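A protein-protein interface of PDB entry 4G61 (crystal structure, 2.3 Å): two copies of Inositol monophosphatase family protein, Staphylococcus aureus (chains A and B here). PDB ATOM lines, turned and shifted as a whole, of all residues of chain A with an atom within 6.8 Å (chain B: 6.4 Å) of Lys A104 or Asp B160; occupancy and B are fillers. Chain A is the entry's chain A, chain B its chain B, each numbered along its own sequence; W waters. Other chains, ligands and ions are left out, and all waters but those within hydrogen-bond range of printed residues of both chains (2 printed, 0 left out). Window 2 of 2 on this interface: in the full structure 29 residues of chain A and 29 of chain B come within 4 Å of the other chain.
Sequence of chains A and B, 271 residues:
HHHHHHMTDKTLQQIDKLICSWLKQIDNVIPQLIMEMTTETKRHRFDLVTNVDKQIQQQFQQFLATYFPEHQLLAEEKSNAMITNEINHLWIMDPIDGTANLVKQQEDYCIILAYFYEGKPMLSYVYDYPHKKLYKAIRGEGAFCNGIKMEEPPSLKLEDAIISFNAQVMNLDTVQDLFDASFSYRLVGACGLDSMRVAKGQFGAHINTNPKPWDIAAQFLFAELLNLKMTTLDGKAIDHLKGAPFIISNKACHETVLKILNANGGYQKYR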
ATOM      1  N   MET A  37     -32.041 -39.712  32.980  1.00  0.00           N
ATOM      2  CA  MET A  37     -30.958 -39.621  31.988  1.00  0.00           C
ATOM      3  C   MET A  37     -29.672 -40.263  32.514  1.00  0.00           C
ATOM      4  O   MET A  37     -29.228 -39.961  33.629  1.00  0.00           O
ATOM      5  CB  MET A  37     -30.741 -38.159  31.570  1.00  0.00           C
ATOM      6  CG  MET A  37     -29.452 -37.813  30.850  1.00  0.00           C
ATOM      7  SD  MET A  37     -29.435 -36.307  29.827  1.00  0.00           S
ATOM      8  CE  MET A  37     -30.310 -35.026  30.711  1.00  0.00           C
ATOM      9  N   ARG A  45     -13.805 -39.455  26.036  1.00  0.00           N
ATOM     10  CA  ARG A  45     -14.551 -39.102  27.214  1.00  0.00           C
ATOM     11  C   ARG A  45     -15.659 -38.070  27.017  1.00  0.00           C
ATOM     12  O   ARG A  45     -16.634 -38.059  27.757  1.00  0.00           O
ATOM     13  CB  ARG A  45     -13.608 -38.675  28.341  1.00  0.00           C
ATOM     14  CG  ARG A  45     -13.973 -39.417  29.630  1.00  0.00           C
ATOM     15  CD  ARG A  45     -13.361 -38.845  30.863  1.00  0.00           C
ATOM     16  NE  ARG A  45     -13.851 -37.497  31.159  1.00  0.00           N
ATOM     17  CZ  ARG A  45     -13.094 -36.581  31.748  1.00  0.00           C
ATOM     18  NH1 ARG A  45     -11.858 -36.908  32.078  1.00  0.00           N
ATOM     19  NH2 ARG A  45     -13.556 -35.363  32.013  1.00  0.00           N
ATOM     20  N   PHE A  46     -15.525 -37.196  26.024  1.00  0.00           N
ATOM     21  CA  PHE A  46     -16.580 -36.207  25.764  1.00  0.00           C
ATOM     22  C   PHE A  46     -17.513 -36.527  24.546  1.00  0.00           C
ATOM     23  O   PHE A  46     -18.344 -35.700  24.149  1.00  0.00           O
ATOM     24  CB  PHE A  46     -15.959 -34.795  25.652  1.00  0.00           C
ATOM     25  CG  PHE A  46     -15.575 -34.160  27.016  1.00  0.00           C
ATOM     26  CD1 PHE A  46     -16.091 -34.672  28.239  1.00  0.00           C
ATOM     27  CD2 PHE A  46     -14.741 -33.024  27.065  1.00  0.00           C
ATOM     28  CE1 PHE A  46     -15.746 -34.095  29.490  1.00  0.00           C
ATOM     29  CE2 PHE A  46     -14.391 -32.401  28.315  1.00  0.00           C
ATOM     30  CZ  PHE A  46     -14.887 -32.934  29.516  1.00  0.00           C
ATOM     31  N   LEU A  48     -20.479 -38.214  23.728  1.00  0.00           N
ATOM     32  CA  LEU A  48     -21.522 -38.727  24.609  1.00  0.00           C
ATOM     33  C   LEU A  48     -22.663 -39.392  23.878  1.00  0.00           C
ATOM     34  O   LEU A  48     -23.091 -38.955  22.794  1.00  0.00           O
ATOM     35  CB  LEU A  48     -22.122 -37.569  25.393  1.00  0.00           C
ATOM     36  CG  LEU A  48     -21.517 -37.119  26.727  1.00  0.00           C
ATOM     37  CD1 LEU A  48     -20.090 -37.522  26.988  1.00  0.00           C
ATOM     38  CD2 LEU A  48     -21.762 -35.635  26.959  1.00  0.00           C
ATOM     39  N   THR A  99     -26.199 -33.959  21.425  1.00  0.00           N
ATOM     40  CA  THR A  99     -26.268 -34.683  22.712  1.00  0.00           C
ATOM     41  C   THR A  99     -25.559 -33.856  23.813  1.00  0.00           C
ATOM     42  O   THR A  99     -26.019 -33.771  24.950  1.00  0.00           O
ATOM     43  CB  THR A  99     -25.644 -36.103  22.576  1.00  0.00           C
ATOM     44  OG1 THR A  99     -26.252 -36.750  21.450  1.00  0.00           O
ATOM     45  CG2 THR A  99     -25.902 -36.903  23.772  1.00  0.00           C
ATOM     46  N   ALA A 100     -24.439 -33.223  23.476  1.00  0.00           N
ATOM     47  CA  ALA A 100     -23.755 -32.474  24.483  1.00  0.00           C
ATOM     48  C   ALA A 100     -24.747 -31.401  25.043  1.00  0.00           C
ATOM     49  O   ALA A 100     -24.860 -31.203  26.245  1.00  0.00           O
ATOM     50  CB  ALA A 100     -22.490 -31.873  23.888  1.00  0.00           C
ATOM     51  N   ASN A 101     -25.483 -30.733  24.160  1.00  0.00           N
ATOM     52  CA  ASN A 101     -26.465 -29.745  24.582  1.00  0.00           C
ATOM     53  C   ASN A 101     -27.552 -30.396  25.377  1.00  0.00           C
ATOM     54  O   ASN A 101     -27.918 -29.897  26.447  1.00  0.00           O
ATOM     55  CB  ASN A 101     -27.055 -29.042  23.385  1.00  0.00           C
ATOM     56  CG  ASN A 101     -26.165 -27.949  22.855  1.00  0.00           C
ATOM     57  OD1 ASN A 101     -25.217 -27.528  23.504  1.00  0.00           O
ATOM     58  ND2 ASN A 101     -26.433 -27.522  21.648  1.00  0.00           N
ATOM     59  N   LEU A 102     -28.065 -31.537  24.925  1.00  0.00           N
ATOM     60  CA  LEU A 102     -29.044 -32.271  25.766  1.00  0.00           C
ATOM     61  C   LEU A 102     -28.492 -32.475  27.185  1.00  0.00           C
ATOM     62  O   LEU A 102     -29.147 -32.148  28.182  1.00  0.00           O
ATOM     63  CB  LEU A 102     -29.348 -33.625  25.143  1.00  0.00           C
ATOM     64  CG  LEU A 102     -30.079 -34.617  26.029  1.00  0.00           C
ATOM     65  CD1 LEU A 102     -31.526 -34.158  26.215  1.00  0.00           C
ATOM     66  CD2 LEU A 102     -30.009 -35.976  25.349  1.00  0.00           C
ATOM     67  N   VAL A 103     -27.267 -33.003  27.279  1.00  0.00           N
ATOM     68  CA  VAL A 103     -26.709 -33.306  28.583  1.00  0.00           C
ATOM     69  C   VAL A 103     -26.492 -32.057  29.450  1.00  0.00           C
ATOM     70  O   VAL A 103     -26.849 -32.068  30.609  1.00  0.00           O
ATOM     71  CB  VAL A 103     -25.404 -34.110  28.465  1.00  0.00           C
ATOM     72  CG1 VAL A 103     -24.784 -34.355  29.869  1.00  0.00           C
ATOM     73  CG2 VAL A 103     -25.671 -35.455  27.690  1.00  0.00           C
ATOM     74  N   LYS A 104     -25.885 -30.999  28.884  1.00  0.00           N
ATOM     75  CA  LYS A 104     -25.433 -29.850  29.692  1.00  0.00           C
ATOM     76  C   LYS A 104     -26.523 -28.798  29.897  1.00  0.00           C
ATOM     77  O   LYS A 104     -26.553 -28.074  30.909  1.00  0.00           O
ATOM     78  CB  LYS A 104     -24.190 -29.213  29.064  1.00  0.00           C
ATOM     79  CG  LYS A 104     -22.930 -30.123  29.037  1.00  0.00           C
ATOM     80  CD  LYS A 104     -22.460 -30.530  30.461  1.00  0.00           C
ATOM     81  CE  LYS A 104     -21.441 -31.692  30.381  1.00  0.00           C
ATOM     82  NZ  LYS A 104     -20.479 -31.751  31.565  1.00  0.00           N
ATOM     83  N   GLN A 105     -27.444 -28.759  28.942  1.00  0.00           N
ATOM     84  CA  GLN A 105     -28.421 -27.707  28.903  1.00  0.00           C
ATOM     85  C   GLN A 105     -29.877 -28.181  28.835  1.00  0.00           C
ATOM     86  O   GLN A 105     -30.767 -27.416  29.200  1.00  0.00           O
ATOM     87  CB  GLN A 105     -28.166 -26.796  27.700  1.00  0.00           C
ATOM     88  CG  GLN A 105     -26.725 -26.373  27.432  1.00  0.00           C
ATOM     89  CD  GLN A 105     -26.685 -25.185  26.475  1.00  0.00           C
ATOM     90  OE1 GLN A 105     -27.144 -24.111  26.830  1.00  0.00           O
ATOM     91  NE2 GLN A 105     -26.147 -25.380  25.261  1.00  0.00           N
ATOM     92  N   GLN A 106     -30.131 -29.385  28.323  1.00  0.00           N
ATOM     93  CA  GLN A 106     -31.480 -29.820  28.017  1.00  0.00           C
ATOM     94  C   GLN A 106     -32.200 -28.782  27.141  1.00  0.00           C
ATOM     95  O   GLN A 106     -33.419 -28.507  27.295  1.00  0.00           O
ATOM     96  CB  GLN A 106     -32.271 -30.110  29.284  1.00  0.00           C
ATOM     97  CG  GLN A 106     -31.900 -31.414  29.909  1.00  0.00           C
ATOM     98  CD  GLN A 106     -31.755 -31.240  31.373  1.00  0.00           C
ATOM     99  OE1 GLN A 106     -31.097 -30.263  31.826  1.00  0.00           O
ATOM    100  NE2 GLN A 106     -32.373 -32.136  32.152  1.00  0.00           N
ATOM    101  N   GLU A 107     -31.455 -28.281  26.172  1.00  0.00           N
ATOM    102  CA  GLU A 107     -31.949 -27.281  25.292  1.00  0.00           C
ATOM    103  C   GLU A 107     -31.013 -27.266  24.101  1.00  0.00           C
ATOM    104  O   GLU A 107     -29.831 -27.662  24.215  1.00  0.00           O
ATOM    105  CB  GLU A 107     -31.943 -25.909  26.012  1.00  0.00           C
ATOM    106  CG  GLU A 107     -32.814 -24.916  25.290  1.00  0.00           C
ATOM    107  CD  GLU A 107     -33.047 -23.596  26.052  1.00  0.00           C
ATOM    108  OE1 GLU A 107     -32.972 -23.515  27.292  1.00  0.00           O
ATOM    109  OE2 GLU A 107     -33.375 -22.626  25.363  1.00  0.00           O
ATOM    110  N   LEU B 156     -20.508 -26.524  39.007  1.00  0.00           N
ATOM    111  CA  LEU B 156     -19.852 -26.863  37.748  1.00  0.00           C
ATOM    112  C   LEU B 156     -18.409 -26.407  37.782  1.00  0.00           C
ATOM    113  O   LEU B 156     -18.132 -25.197  37.822  1.00  0.00           O
ATOM    114  CB  LEU B 156     -20.548 -26.164  36.557  1.00  0.00           C
ATOM    115  CG  LEU B 156     -21.918 -26.696  36.102  1.00  0.00           C
ATOM    116  CD1 LEU B 156     -22.576 -25.828  35.076  1.00  0.00           C
ATOM    117  CD2 LEU B 156     -21.774 -28.130  35.551  1.00  0.00           C
ATOM    118  N   LYS B 157     -17.498 -27.362  37.712  1.00  0.00           N
ATOM    119  CA  LYS B 157     -16.095 -27.100  37.413  1.00  0.00           C
ATOM    120  C   LYS B 157     -15.931 -26.839  35.944  1.00  0.00           C
ATOM    121  O   LYS B 157     -16.727 -27.335  35.125  1.00  0.00           O
ATOM    122  CB  LYS B 157     -15.246 -28.330  37.763  1.00  0.00           C
ATOM    123  CG  LYS B 157     -15.012 -28.554  39.256  1.00  0.00           C
ATOM    124  CD  LYS B 157     -15.189 -30.045  39.586  1.00  0.00           C
ATOM    125  CE  LYS B 157     -14.493 -31.012  38.609  1.00  0.00           C
ATOM    126  NZ  LYS B 157     -14.597 -32.420  39.115  1.00  0.00           N
ATOM    127  N   LEU B 158     -14.873 -26.094  35.606  1.00  0.00           N
ATOM    128  CA  LEU B 158     -14.715 -25.515  34.279  1.00  0.00           C
ATOM    129  C   LEU B 158     -14.757 -26.586  33.217  1.00  0.00           C
ATOM    130  O   LEU B 158     -15.417 -26.420  32.205  1.00  0.00           O
ATOM    131  CB  LEU B 158     -13.422 -24.676  34.142  1.00  0.00           C
ATOM    132  CG  LEU B 158     -13.361 -23.877  32.827  1.00  0.00           C
ATOM    133  CD1 LEU B 158     -14.717 -23.287  32.466  1.00  0.00           C
ATOM    134  CD2 LEU B 158     -12.326 -22.763  32.795  1.00  0.00           C
ATOM    135  N   GLU B 159     -14.084 -27.697  33.494  1.00  0.00           N
ATOM    136  CA  GLU B 159     -13.895 -28.731  32.511  1.00  0.00           C
ATOM    137  C   GLU B 159     -15.185 -29.500  32.218  1.00  0.00           C
ATOM    138  O   GLU B 159     -15.231 -30.267  31.282  1.00  0.00           O
ATOM    139  CB  GLU B 159     -12.783 -29.677  32.967  1.00  0.00           C
ATOM    140  CG  GLU B 159     -13.044 -30.366  34.303  1.00  0.00           C
ATOM    141  CD  GLU B 159     -12.385 -29.641  35.507  1.00  0.00           C
ATOM    142  OE1 GLU B 159     -12.038 -30.384  36.466  1.00  0.00           O
ATOM    143  OE2 GLU B 159     -12.208 -28.382  35.523  1.00  0.00           O
ATOM    144  N   ASP B 160     -16.208 -29.272  33.043  1.00  0.00           N
ATOM    145  CA  ASP B 160     -17.532 -29.843  32.867  1.00  0.00           C
ATOM    146  C   ASP B 160     -18.526 -28.823  32.334  1.00  0.00           C
ATOM    147  O   ASP B 160     -19.692 -29.169  32.166  1.00  0.00           O
ATOM    148  CB  ASP B 160     -18.024 -30.373  34.209  1.00  0.00           C
ATOM    149  CG  ASP B 160     -17.219 -31.588  34.670  1.00  0.00           C
ATOM    150  OD1 ASP B 160     -16.901 -32.471  33.820  1.00  0.00           O
ATOM    151  OD2 ASP B 160     -16.892 -31.661  35.866  1.00  0.00           O
ATOM    152  N   ALA B 161     -18.078 -27.594  32.059  1.00  0.00           N
ATOM    153  CA  ALA B 161     -19.006 -26.486  31.784  1.00  0.00           C
ATOM    154  C   ALA B 161     -18.903 -26.016  30.349  1.00  0.00           C
ATOM    155  O   ALA B 161     -17.822 -26.001  29.781  1.00  0.00           O
ATOM    156  CB  ALA B 161     -18.755 -25.279  32.720  1.00  0.00           C
ATOM    157  N   ILE B 162     -20.026 -25.632  29.781  1.00  0.00           N
ATOM    158  CA  ILE B 162     -20.002 -24.901  28.528  1.00  0.00           C
ATOM    159  C   ILE B 162     -19.744 -23.477  28.896  1.00  0.00           C
ATOM    160  O   ILE B 162     -20.332 -22.976  29.853  1.00  0.00           O
ATOM    161  CB  ILE B 162     -21.338 -24.977  27.777  1.00  0.00           C
ATOM    162  CG1 ILE B 162     -21.529 -26.370  27.180  1.00  0.00           C
ATOM    163  CG2 ILE B 162     -21.418 -23.867  26.743  1.00  0.00           C
ATOM    164  CD1 ILE B 162     -22.918 -26.582  26.504  1.00  0.00           C
ATOM    165  N   ALA B 181      -9.750 -25.521  28.471  1.00  0.00           N
ATOM    166  CA  ALA B 181     -10.094 -25.813  29.859  1.00  0.00           C
ATOM    167  C   ALA B 181     -11.598 -26.130  30.041  1.00  0.00           C
ATOM    168  O   ALA B 181     -11.997 -26.651  31.065  1.00  0.00           O
ATOM    169  CB  ALA B 181      -9.682 -24.685  30.781  1.00  0.00           C
ATOM    170  N   SER B 182     -12.436 -25.775  29.081  1.00  0.00           N
ATOM    171  CA  SER B 182     -13.844 -25.951  29.347  1.00  0.00           C
ATOM    172  C   SER B 182     -14.425 -27.148  28.612  1.00  0.00           C
ATOM    173  O   SER B 182     -13.725 -27.854  27.892  1.00  0.00           O
ATOM    174  CB  SER B 182     -14.590 -24.674  29.016  1.00  0.00           C
ATOM    175  OG  SER B 182     -14.259 -24.327  27.726  1.00  0.00           O
ATOM    176  N   PHE B 183     -15.698 -27.432  28.842  1.00  0.00           N
ATOM    177  CA  PHE B 183     -16.246 -28.632  28.242  1.00  0.00           C
ATOM    178  C   PHE B 183     -16.559 -28.323  26.773  1.00  0.00           C
ATOM    179  O   PHE B 183     -16.237 -29.135  25.887  1.00  0.00           O
ATOM    180  CB  PHE B 183     -17.467 -29.141  29.018  1.00  0.00           C
ATOM    181  CG  PHE B 183     -18.238 -30.206  28.280  1.00  0.00           C
ATOM    182  CD1 PHE B 183     -17.922 -31.541  28.445  1.00  0.00           C
ATOM    183  CD2 PHE B 183     -19.237 -29.851  27.378  1.00  0.00           C
ATOM    184  CE1 PHE B 183     -18.617 -32.508  27.744  1.00  0.00           C
ATOM    185  CE2 PHE B 183     -19.919 -30.820  26.627  1.00  0.00           C
ATOM    186  CZ  PHE B 183     -19.609 -32.137  26.805  1.00  0.00           C
ATOM    187  N   SER B 184     -17.193 -27.171  26.514  1.00  0.00           N
ATOM    188  CA  SER B 184     -17.372 -26.702  25.141  1.00  0.00           C
ATOM    189  C   SER B 184     -17.678 -25.217  25.097  1.00  0.00           C
ATOM    190  O   SER B 184     -17.712 -24.539  26.122  1.00  0.00           O
ATOM    191  CB  SER B 184     -18.457 -27.498  24.392  1.00  0.00           C
ATOM    192  OG  SER B 184     -18.289 -27.299  22.987  1.00  0.00           O
ATOM    193  N   GLY B 201     -27.708 -22.721  35.058  1.00  0.00           N
ATOM    194  CA  GLY B 201     -26.848 -23.895  35.092  1.00  0.00           C
ATOM    195  C   GLY B 201     -26.597 -24.598  33.756  1.00  0.00           C
ATOM    196  O   GLY B 201     -25.964 -25.643  33.712  1.00  0.00           O
ATOM    197  N   GLN B 202     -27.042 -23.992  32.660  1.00  0.00           N
ATOM    198  CA  GLN B 202     -26.739 -24.510  31.341  1.00  0.00           C
ATOM    199  C   GLN B 202     -25.330 -24.148  30.895  1.00  0.00           C
ATOM    200  O   GLN B 202     -24.719 -24.904  30.165  1.00  0.00           O
ATOM    201  CB  GLN B 202     -27.752 -23.980  30.361  1.00  0.00           C
ATOM    202  CG  GLN B 202     -29.199 -24.240  30.812  1.00  0.00           C
ATOM    203  CD  GLN B 202     -30.220 -23.499  29.960  1.00  0.00           C
ATOM    204  OE1 GLN B 202     -30.349 -22.300  30.060  1.00  0.00           O
ATOM    205  NE2 GLN B 202     -30.924 -24.218  29.092  1.00  0.00           N
ATOM    206  N   PHE B 203     -24.825 -23.002  31.332  1.00  0.00           N
ATOM    207  CA  PHE B 203     -23.447 -22.568  31.067  1.00  0.00           C
ATOM    208  C   PHE B 203     -22.769 -22.465  32.442  1.00  0.00           C
ATOM    209  O   PHE B 203     -23.452 -22.316  33.502  1.00  0.00           O
ATOM    210  CB  PHE B 203     -23.388 -21.155  30.421  1.00  0.00           C
ATOM    211  CG  PHE B 203     -23.864 -21.075  28.948  1.00  0.00           C
ATOM    212  CD1 PHE B 203     -24.073 -22.222  28.156  1.00  0.00           C
ATOM    213  CD2 PHE B 203     -24.023 -19.837  28.355  1.00  0.00           C
ATOM    214  CE1 PHE B 203     -24.492 -22.097  26.809  1.00  0.00           C
ATOM    215  CE2 PHE B 203     -24.426 -19.706  27.018  1.00  0.00           C
ATOM    216  CZ  PHE B 203     -24.672 -20.834  26.248  1.00  0.00           C
HETATM  217  O   HOH W   1     -18.434 -33.384  31.968  1.00  0.00           O
HETATM  218  O   HOH W   2     -24.435 -27.647  32.583  1.00  0.00           O
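Printed residues of chain B within 4 Å of Ala A100: Phe B183. Of the printed residues of chain B, Lys A104 touches Asp B160, Ile B162, Phe B183, Gly B201 and Gln B202. Asp B160 touches one residue of chain A. Ala B161 touches none of the printed residues of chain A. Ser B182 touches none of the printed residues of chain A. Printed residues of chain A within 4 Å of Phe B183: Phe A46, Ala A100 and Lys A104. Printed residues of chain A within 4 Å of Gln B202: Lys A104, Gln A105 and Glu A107. The nearest printed residue of chain B that does not touch Glu A107 is Ile B162 (7.4 Å).
The backbone NH of Phe B183 is in hydrogen-bond range of the backbone carbonyl oxygen of Ala B161 (2.7 Å). O of Ala B181 sits close to N of Glu B159 (3.4 Å). The side-chain amide oxygen of Asn A101 lies within hydrogen-bond range of the side-chain amide nitrogen of Gln A105 (2.9 Å). The backbone carbonyl oxygen of Asn A101 is in hydrogen-bond range of the backbone NH of Gln A106, at 2.9 Å.
Phe A46 touches Glu B159. Phe B183 touches Phe A46. Ala A100 touches Phe B183. Asn A101 touches Ile B162. CB of Lys A104 touches CD1 of Ile B162, at 3.9 Å. Phe B183 touches Lys A104. Lys A104 touches Gly B201 (O to O, 3.8 Å). Lys A104 touches Gln B202. Gln A105 touches Ile B162 (NE2 to CD1, 3.7 Å). Phe B203 touches Gln A105 (CE1 to OE1, 3.3 Å).
Of the 14 printed residues of chain B, 7 touch a printed residue of chain A. Hydrophobic or aromatic side chains of chain A that line the printed part of chain B: Phe A46 and Ala A100. Among the printed residues, 13 pairs touch across the chains.
Water W1 bridges OD1 of Asp B160 (2.6 Å) and NZ of Lys A104 (2.6 Å). Water W2 lies within hydrogen-bond range of O of Lys A104 and O of Gly B201.
The backbone carbonyl oxygen (O) of Gln A105 is in hydrogen-bond range of the side-chain amide nitrogen (NE2) of Gln B202 (3.2 Å). The side-chain amino group of Lys A104 sits at hydrogen-bond distance from the backbone carbonyl oxygen of Asp B160, 2.8 Å away. OE1 of Glu A107 is in hydrogen-bond range of NE2 of Gln B202, 2.8 Å away.
No position is printed for both chains.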
